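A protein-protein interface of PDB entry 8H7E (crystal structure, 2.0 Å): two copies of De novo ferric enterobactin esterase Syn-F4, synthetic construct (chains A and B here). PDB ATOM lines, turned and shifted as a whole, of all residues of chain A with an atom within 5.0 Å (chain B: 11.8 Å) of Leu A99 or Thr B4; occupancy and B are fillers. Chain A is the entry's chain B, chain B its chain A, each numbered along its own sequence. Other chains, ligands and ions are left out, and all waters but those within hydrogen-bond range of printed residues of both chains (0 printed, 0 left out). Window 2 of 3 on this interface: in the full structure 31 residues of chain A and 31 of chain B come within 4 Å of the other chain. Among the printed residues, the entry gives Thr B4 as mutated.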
ATOM      1  N   LEU A   5      16.962 -30.230 -33.825  1.00  0.00           N
ATOM      2  CA  LEU A   5      18.304 -30.319 -33.267  1.00  0.00           C
ATOM      3  C   LEU A   5      19.365 -29.960 -34.308  1.00  0.00           C
ATOM      4  O   LEU A   5      20.273 -29.180 -34.031  1.00  0.00           O
ATOM      5  CB  LEU A   5      18.530 -31.746 -32.715  1.00  0.00           C
ATOM      6  CG  LEU A   5      18.933 -31.897 -31.249  1.00  0.00           C
ATOM      7  CD1 LEU A   5      17.860 -31.322 -30.342  1.00  0.00           C
ATOM      8  CD2 LEU A   5      19.157 -33.368 -30.934  1.00  0.00           C
ATOM      9  N   GLN A  95      29.222 -31.289 -28.802  1.00  0.00           N
ATOM     10  CA  GLN A  95      28.149 -32.045 -28.153  1.00  0.00           C
ATOM     11  C   GLN A  95      26.883 -32.079 -28.998  1.00  0.00           C
ATOM     12  O   GLN A  95      26.261 -33.140 -29.180  1.00  0.00           O
ATOM     13  CB  GLN A  95      27.803 -31.450 -26.788  1.00  0.00           C
ATOM     14  CG  GLN A  95      28.914 -31.519 -25.743  1.00  0.00           C
ATOM     15  CD  GLN A  95      28.615 -30.666 -24.510  1.00  0.00           C
ATOM     16  OE1 GLN A  95      27.500 -30.171 -24.349  1.00  0.00           O
ATOM     17  NE2 GLN A  95      29.607 -30.493 -23.634  1.00  0.00           N
ATOM     18  N   LEU A  96      26.503 -30.911 -29.515  1.00  0.00           N
ATOM     19  CA  LEU A  96      25.370 -30.822 -30.438  1.00  0.00           C
ATOM     20  C   LEU A  96      25.537 -31.674 -31.680  1.00  0.00           C
ATOM     21  O   LEU A  96      24.632 -32.426 -32.057  1.00  0.00           O
ATOM     22  CB  LEU A  96      25.132 -29.368 -30.876  1.00  0.00           C
ATOM     23  CG  LEU A  96      24.027 -28.647 -30.147  1.00  0.00           C
ATOM     24  CD1 LEU A  96      23.999 -27.198 -30.608  1.00  0.00           C
ATOM     25  CD2 LEU A  96      22.693 -29.326 -30.431  1.00  0.00           C
ATOM     26  N   ASP A  97      26.684 -31.514 -32.336  1.00  0.00           N
ATOM     27  CA  ASP A  97      27.065 -32.358 -33.473  1.00  0.00           C
ATOM     28  C   ASP A  97      26.858 -33.860 -33.195  1.00  0.00           C
ATOM     29  O   ASP A  97      26.260 -34.561 -33.998  1.00  0.00           O
ATOM     30  CB  ASP A  97      28.531 -32.094 -33.846  1.00  0.00           C
ATOM     31  CG  ASP A  97      28.896 -32.602 -35.222  1.00  0.00           C
ATOM     32  OD1 ASP A  97      28.015 -33.043 -35.994  1.00  0.00           O
ATOM     33  OD2 ASP A  97      30.091 -32.533 -35.547  1.00  0.00           O
ATOM     34  N   ASN A  98      27.361 -34.339 -32.066  1.00  0.00           N
ATOM     35  CA  ASN A  98      27.250 -35.759 -31.710  1.00  0.00           C
ATOM     36  C   ASN A  98      25.798 -36.202 -31.534  1.00  0.00           C
ATOM     37  O   ASN A  98      25.393 -37.263 -32.031  1.00  0.00           O
ATOM     38  CB  ASN A  98      28.040 -36.064 -30.431  1.00  0.00           C
ATOM     39  CG  ASN A  98      27.871 -37.515 -29.979  1.00  0.00           C
ATOM     40  OD1 ASN A  98      28.125 -38.449 -30.761  1.00  0.00           O
ATOM     41  ND2 ASN A  98      27.395 -37.712 -28.732  1.00  0.00           N
ATOM     42  N   LEU A  99      25.031 -35.368 -30.823  1.00  0.00           N
ATOM     43  CA  LEU A  99      23.604 -35.596 -30.568  1.00  0.00           C
ATOM     44  C   LEU A  99      22.781 -35.701 -31.856  1.00  0.00           C
ATOM     45  O   LEU A  99      21.921 -36.569 -31.952  1.00  0.00           O
ATOM     46  CB  LEU A  99      23.041 -34.480 -29.675  1.00  0.00           C
ATOM     47  CG  LEU A  99      22.314 -34.844 -28.379  1.00  0.00           C
ATOM     48  CD1 LEU A  99      23.012 -35.928 -27.579  1.00  0.00           C
ATOM     49  CD2 LEU A  99      22.184 -33.591 -27.533  1.00  0.00           C
ATOM     50  N   VAL A 100      23.031 -34.822 -32.832  1.00  0.00           N
ATOM     51  CA  VAL A 100      22.257 -34.836 -34.098  1.00  0.00           C
ATOM     52  C   VAL A 100      22.600 -36.026 -34.997  1.00  0.00           C
ATOM     53  O   VAL A 100      21.740 -36.528 -35.731  1.00  0.00           O
ATOM     54  CB  VAL A 100      22.370 -33.532 -34.940  1.00  0.00           C
ATOM     55  CG1 VAL A 100      21.916 -32.331 -34.143  1.00  0.00           C
ATOM     56  CG2 VAL A 100      23.770 -33.286 -35.474  1.00  0.00           C
ATOM     57  N   HIS A 101      23.852 -36.484 -34.925  1.00  0.00           N
ATOM     58  CA  HIS A 101      24.324 -37.567 -35.773  1.00  0.00           C
ATOM     59  C   HIS A 101      24.311 -38.898 -35.035  1.00  0.00           C
ATOM     60  O   HIS A 101      25.024 -39.819 -35.416  1.00  0.00           O
ATOM     61  CB  HIS A 101      25.715 -37.209 -36.304  1.00  0.00           C
ATOM     62  CG  HIS A 101      25.697 -36.067 -37.261  1.00  0.00           C
ATOM     63  ND1 HIS A 101      26.378 -34.892 -37.039  1.00  0.00           N
ATOM     64  CD2 HIS A 101      25.042 -35.908 -38.434  1.00  0.00           C
ATOM     65  CE1 HIS A 101      26.164 -34.068 -38.050  1.00  0.00           C
ATOM     66  NE2 HIS A 101      25.354 -34.658 -38.906  1.00  0.00           N
ATOM     67  N   ARG A 102      23.452 -39.009 -34.019  1.00  0.00           N
ATOM     68  CA  ARG A 102      23.540 -40.065 -33.013  1.00  0.00           C
ATOM     69  C   ARG A 102      22.867 -41.347 -33.474  1.00  0.00           C
ATOM     70  O   ARG A 102      22.963 -42.374 -32.794  1.00  0.00           O
ATOM     71  CB  ARG A 102      22.915 -39.577 -31.694  1.00  0.00           C
ATOM     72  CG  ARG A 102      23.362 -40.287 -30.425  1.00  0.00           C
ATOM     73  CD  ARG A 102      24.866 -40.204 -30.222  1.00  0.00           C
ATOM     74  NE  ARG A 102      25.305 -40.936 -29.039  1.00  0.00           N
ATOM     75  CZ  ARG A 102      26.579 -41.159 -28.708  1.00  0.00           C
ATOM     76  NH1 ARG A 102      27.574 -40.719 -29.470  1.00  0.00           N
ATOM     77  NH2 ARG A 102      26.860 -41.828 -27.597  1.00  0.00           N
ATOM     78  OXT ARG A 102      22.225 -41.393 -34.528  1.00  0.00           O
ATOM     79  N   GLY B   3      18.090 -34.174 -18.811  1.00  0.00           N
ATOM     80  CA  GLY B   3      18.969 -34.846 -19.823  1.00  0.00           C
ATOM     81  C   GLY B   3      20.194 -34.023 -20.193  1.00  0.00           C
ATOM     82  O   GLY B   3      20.535 -33.045 -19.513  1.00  0.00           O
ATOM     83  N   THR B   4      20.863 -34.430 -21.269  1.00  0.00           N
ATOM     84  CA  THR B   4      22.068 -33.743 -21.731  1.00  0.00           C
ATOM     85  C   THR B   4      21.717 -32.479 -22.557  1.00  0.00           C
ATOM     86  O   THR B   4      22.553 -31.605 -22.715  1.00  0.00           O
ATOM     87  CB  THR B   4      23.033 -34.709 -22.478  1.00  0.00           C
ATOM     88  OG1 THR B   4      24.366 -34.183 -22.441  1.00  0.00           O
ATOM     89  CG2 THR B   4      22.619 -34.955 -23.926  1.00  0.00           C
ATOM     90  N   LEU B   5      20.484 -32.395 -23.057  1.00  0.00           N
ATOM     91  CA  LEU B   5      19.978 -31.179 -23.719  1.00  0.00           C
ATOM     92  C   LEU B   5      19.724 -30.057 -22.699  1.00  0.00           C
ATOM     93  O   LEU B   5      19.925 -28.874 -22.989  1.00  0.00           O
ATOM     94  CB  LEU B   5      18.697 -31.482 -24.515  1.00  0.00           C
ATOM     95  CG  LEU B   5      18.621 -30.953 -25.955  1.00  0.00           C
ATOM     96  CD1 LEU B   5      19.652 -31.604 -26.853  1.00  0.00           C
ATOM     97  CD2 LEU B   5      17.242 -31.183 -26.543  1.00  0.00           C
ATOM     98  N   ASN B   6      19.315 -30.445 -21.498  1.00  0.00           N
ATOM     99  CA  ASN B   6      19.128 -29.507 -20.412  1.00  0.00           C
ATOM    100  C   ASN B   6      20.456 -28.850 -20.022  1.00  0.00           C
ATOM    101  O   ASN B   6      20.494 -27.631 -19.823  1.00  0.00           O
ATOM    102  CB  ASN B   6      18.497 -30.190 -19.192  1.00  0.00           C
ATOM    103  CG  ASN B   6      17.302 -31.068 -19.553  1.00  0.00           C
ATOM    104  OD1 ASN B   6      17.444 -32.055 -20.304  1.00  0.00           O
ATOM    105  ND2 ASN B   6      16.123 -30.733 -19.017  1.00  0.00           N
ATOM    106  N   GLN B   7      21.534 -29.638 -19.942  1.00  0.00           N
ATOM    107  CA  GLN B   7      22.875 -29.086 -19.677  1.00  0.00           C
ATOM    108  C   GLN B   7      23.406 -28.278 -20.844  1.00  0.00           C
ATOM    109  O   GLN B   7      24.152 -27.322 -20.623  1.00  0.00           O
ATOM    110  CB  GLN B   7      23.920 -30.139 -19.250  1.00  0.00           C
ATOM    111  CG  GLN B   7      24.430 -31.078 -20.326  1.00  0.00           C
ATOM    112  CD  GLN B   7      25.828 -30.751 -20.860  1.00  0.00           C
ATOM    113  OE1 GLN B   7      26.066 -29.677 -21.431  1.00  0.00           O
ATOM    114  NE2 GLN B   7      26.756 -31.701 -20.709  1.00  0.00           N
ATOM    115  N   LEU B   8      23.049 -28.667 -22.066  1.00  0.00           N
ATOM    116  CA  LEU B   8      23.374 -27.862 -23.221  1.00  0.00           C
ATOM    117  C   LEU B   8      22.783 -26.485 -23.035  1.00  0.00           C
ATOM    118  O   LEU B   8      23.469 -25.494 -23.199  1.00  0.00           O
ATOM    119  CB  LEU B   8      22.787 -28.435 -24.517  1.00  0.00           C
ATOM    120  CG  LEU B   8      23.433 -29.605 -25.245  1.00  0.00           C
ATOM    121  CD1 LEU B   8      22.792 -29.780 -26.609  1.00  0.00           C
ATOM    122  CD2 LEU B   8      24.922 -29.396 -25.379  1.00  0.00           C
ATOM    123  N   PHE B   9      21.492 -26.455 -22.733  1.00  0.00           N
ATOM    124  CA  PHE B   9      20.780 -25.218 -22.538  1.00  0.00           C
ATOM    125  C   PHE B   9      21.382 -24.353 -21.404  1.00  0.00           C
ATOM    126  O   PHE B   9      21.624 -23.176 -21.580  1.00  0.00           O
ATOM    127  CB  PHE B   9      19.301 -25.472 -22.273  1.00  0.00           C
ATOM    128  CG  PHE B   9      18.576 -24.241 -21.874  1.00  0.00           C
ATOM    129  CD1 PHE B   9      18.237 -23.280 -22.831  1.00  0.00           C
ATOM    130  CD2 PHE B   9      18.314 -23.980 -20.534  1.00  0.00           C
ATOM    131  CE1 PHE B   9      17.604 -22.100 -22.455  1.00  0.00           C
ATOM    132  CE2 PHE B   9      17.694 -22.806 -20.161  1.00  0.00           C
ATOM    133  CZ  PHE B   9      17.329 -21.863 -21.122  1.00  0.00           C
ATOM    134  N   HIS B  10      21.595 -24.959 -20.251  1.00  0.00           N
ATOM    135  CA  HIS B  10      22.224 -24.290 -19.092  1.00  0.00           C
ATOM    136  C   HIS B  10      23.564 -23.636 -19.508  1.00  0.00           C
ATOM    137  O   HIS B  10      23.818 -22.455 -19.238  1.00  0.00           O
ATOM    138  CB  HIS B  10      22.436 -25.376 -18.023  1.00  0.00           C
ATOM    139  CG  HIS B  10      23.136 -24.933 -16.780  1.00  0.00           C
ATOM    140  ND1 HIS B  10      24.508 -24.800 -16.708  1.00  0.00           N
ATOM    141  CD2 HIS B  10      22.667 -24.718 -15.527  1.00  0.00           C
ATOM    142  CE1 HIS B  10      24.847 -24.464 -15.476  1.00  0.00           C
ATOM    143  NE2 HIS B  10      23.750 -24.413 -14.739  1.00  0.00           N
ATOM    144  N   ASN B  11      24.396 -24.415 -20.191  1.00  0.00           N
ATOM    145  CA  ASN B  11      25.723 -23.965 -20.586  1.00  0.00           C
ATOM    146  C   ASN B  11      25.625 -22.811 -21.575  1.00  0.00           C
ATOM    147  O   ASN B  11      26.272 -21.786 -21.378  1.00  0.00           O
ATOM    148  CB  ASN B  11      26.518 -25.106 -21.229  1.00  0.00           C
ATOM    149  CG  ASN B  11      26.940 -26.183 -20.231  1.00  0.00           C
ATOM    150  OD1 ASN B  11      26.896 -26.003 -19.025  1.00  0.00           O
ATOM    151  ND2 ASN B  11      27.376 -27.295 -20.751  1.00  0.00           N
ATOM    152  N   LEU B  12      24.817 -22.980 -22.629  1.00  0.00           N
ATOM    153  CA  LEU B  12      24.633 -21.904 -23.609  1.00  0.00           C
ATOM    154  C   LEU B  12      24.037 -20.643 -22.997  1.00  0.00           C
ATOM    155  O   LEU B  12      24.446 -19.539 -23.350  1.00  0.00           O
ATOM    156  CB  LEU B  12      23.763 -22.343 -24.791  1.00  0.00           C
ATOM    157  CG  LEU B  12      23.678 -21.350 -25.950  1.00  0.00           C
ATOM    158  CD1 LEU B  12      25.057 -21.023 -26.514  1.00  0.00           C
ATOM    159  CD2 LEU B  12      22.808 -21.961 -27.048  1.00  0.00           C
ATOM    160  N   ASN B  13      23.084 -20.812 -22.072  1.00  0.00           N
ATOM    161  CA  ASN B  13      22.556 -19.686 -21.297  1.00  0.00           C
ATOM    162  C   ASN B  13      23.646 -18.856 -20.606  1.00  0.00           C
ATOM    163  O   ASN B  13      23.659 -17.633 -20.714  1.00  0.00           O
ATOM    164  CB  ASN B  13      21.530 -20.147 -20.251  1.00  0.00           C
ATOM    165  CG  ASN B  13      20.787 -18.976 -19.633  1.00  0.00           C
ATOM    166  OD1 ASN B  13      20.075 -18.267 -20.337  1.00  0.00           O
ATOM    167  ND2 ASN B  13      21.012 -18.715 -18.362  1.00  0.00           N
ATOM    168  N   LEU B  93      18.226 -19.582 -28.257  1.00  0.00           N
ATOM    169  CA  LEU B  93      18.091 -20.025 -26.856  1.00  0.00           C
ATOM    170  C   LEU B  93      16.672 -20.390 -26.538  1.00  0.00           C
ATOM    171  O   LEU B  93      16.445 -21.368 -25.862  1.00  0.00           O
ATOM    172  CB  LEU B  93      18.536 -18.951 -25.864  1.00  0.00           C
ATOM    173  CG  LEU B  93      19.978 -19.041 -25.405  1.00  0.00           C
ATOM    174  CD1 LEU B  93      20.330 -17.729 -24.706  1.00  0.00           C
ATOM    175  CD2 LEU B  93      20.184 -20.229 -24.457  1.00  0.00           C
ATOM    176  N   LEU B  96      15.962 -23.728 -28.225  1.00  0.00           N
ATOM    177  CA  LEU B  96      16.579 -24.696 -27.315  1.00  0.00           C
ATOM    178  C   LEU B  96      15.756 -24.919 -26.051  1.00  0.00           C
ATOM    179  O   LEU B  96      15.434 -26.071 -25.709  1.00  0.00           O
ATOM    180  CB  LEU B  96      18.005 -24.273 -26.927  1.00  0.00           C
ATOM    181  CG  LEU B  96      18.840 -25.291 -26.123  1.00  0.00           C
ATOM    182  CD1 LEU B  96      18.702 -26.710 -26.653  1.00  0.00           C
ATOM    183  CD2 LEU B  96      20.307 -24.900 -26.137  1.00  0.00           C
ATOM    184  N   ASP B  97      15.412 -23.816 -25.381  1.00  0.00           N
ATOM    185  CA  ASP B  97      14.618 -23.815 -24.132  1.00  0.00           C
ATOM    186  C   ASP B  97      13.304 -24.557 -24.327  1.00  0.00           C
ATOM    187  O   ASP B  97      12.923 -25.404 -23.510  1.00  0.00           O
ATOM    188  CB  ASP B  97      14.318 -22.361 -23.674  1.00  0.00           C
ATOM    189  CG  ASP B  97      13.808 -22.269 -22.232  1.00  0.00           C
ATOM    190  OD1 ASP B  97      13.805 -23.290 -21.512  1.00  0.00           O
ATOM    191  OD2 ASP B  97      13.418 -21.156 -21.804  1.00  0.00           O
ATOM    192  N   LEU B  99      12.633 -26.773 -26.616  1.00  0.00           N
ATOM    193  CA  LEU B  99      12.878 -28.174 -26.916  1.00  0.00           C
ATOM    194  C   LEU B  99      13.227 -28.986 -25.672  1.00  0.00           C
ATOM    195  O   LEU B  99      12.933 -30.176 -25.609  1.00  0.00           O
ATOM    196  CB  LEU B  99      13.979 -28.298 -27.970  1.00  0.00           C
ATOM    197  CG  LEU B  99      14.095 -29.626 -28.710  1.00  0.00           C
ATOM    198  CD1 LEU B  99      12.748 -30.113 -29.239  1.00  0.00           C
ATOM    199  CD2 LEU B  99      15.093 -29.464 -29.847  1.00  0.00           C
ATOM    200  N   VAL B 100      13.854 -28.337 -24.694  1.00  0.00           N
ATOM    201  CA  VAL B 100      14.156 -28.959 -23.409  1.00  0.00           C
ATOM    202  C   VAL B 100      12.883 -29.248 -22.591  1.00  0.00           C
ATOM    203  O   VAL B 100      12.735 -30.367 -22.103  1.00  0.00           O
ATOM    204  CB  VAL B 100      15.176 -28.110 -22.600  1.00  0.00           C
ATOM    205  CG1 VAL B 100      15.300 -28.589 -21.163  1.00  0.00           C
ATOM    206  CG2 VAL B 100      16.536 -28.166 -23.273  1.00  0.00           C
ATOM    207  N   HIS B 101      11.984 -28.259 -22.479  1.00  0.00           N
ATOM    208  CA  HIS B 101      10.823 -28.259 -21.536  1.00  0.00           C
ATOM    209  C   HIS B 101      10.640 -29.493 -20.627  1.00  0.00           C
ATOM    210  O   HIS B 101      10.556 -29.385 -19.399  1.00  0.00           O
ATOM    211  CB  HIS B 101       9.497 -27.917 -22.262  1.00  0.00           C
ATOM    212  CG  HIS B 101       8.886 -29.056 -23.030  1.00  0.00           C
ATOM    213  ND1 HIS B 101       8.227 -30.103 -22.419  1.00  0.00           N
ATOM    214  CD2 HIS B 101       8.790 -29.282 -24.361  1.00  0.00           C
ATOM    215  CE1 HIS B 101       7.780 -30.938 -23.339  1.00  0.00           C
ATOM    216  NE2 HIS B 101       8.110 -30.463 -24.526  1.00  0.00           N
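ND2 of Asn B11 lies within hydrogen-bond range of OE1 of Gln B7 (2.8 Å).
Leu A99 touches just these residues of chain B: Thr B4 (3.8 Å), Leu B5 (3.3 Å) and Leu B8 (3.97 Å). Printed residues of chain A within 4 Å of Thr B4: Leu A99 (3.8 Å). Gln A95 touches just these residues of chain B: Gln B7 (3.3 Å) and Leu B8 (2.9 Å). Of chain B, only Leu B8 (3.9 Å) comes within 4 Å of Leu A96. No residue of chain B comes within 4 Å of Asp A97. No residue of chain B comes within 4 Å of Asn A98. No residue of chain B comes within 4 Å of Val A100. No residue of chain B comes within 4 Å of His A101. No residue of chain B comes within 4 Å of Arg A102. Of the printed residues of chain A, Gln B7 touches Gln A95. Of the printed residues of chain A, Leu B5 touches Leu A5 and Leu A99. Of the printed residues of chain A, Leu B99 touches Leu A5. Of the printed residues of chain B, Leu A5 touches Leu B5 (3.9 Å) and Leu B99 (3.4 Å). The nearest printed residue of chain A that does not touch Thr B4 is Gln A95 (5.4 Å).
Among the printed residues, pairs that only touch across the chains: Leu A5 with Leu B5, Leu A5 with Leu B99, Gln A95 with Leu B8, Leu A96 with Leu B8, Leu A99 with Thr B4, Leu A99 with Leu B5 and Leu A99 with Leu B8.
The side-chain amide oxygen (OE1) of Gln B7 lies close to the side-chain amide oxygen (OE1) of Gln A95 (3.3 Å).
Leu B5 touches its own counterpart, Leu A5. Leu A5 touches Leu B99, and with the chains exchanged Leu A99 touches Leu B5. Of the 8 pairs that touch across the chains among the printed residues, 3 have their exchanged pair printed and touching as well.
Of the 17 printed residues of chain B, 5 touch a printed residue of chain A. Hydrophobic or aromatic side chains of chain B that line the printed part of chain A: Leu B5, Leu B8 and Leu B99. Among the printed residues, 8 pairs touch across the chains. Among the printed residues, no Asp or Glu carboxylate lies within 4 Å of a Lys or Arg side-chain nitrogen of the other chain.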
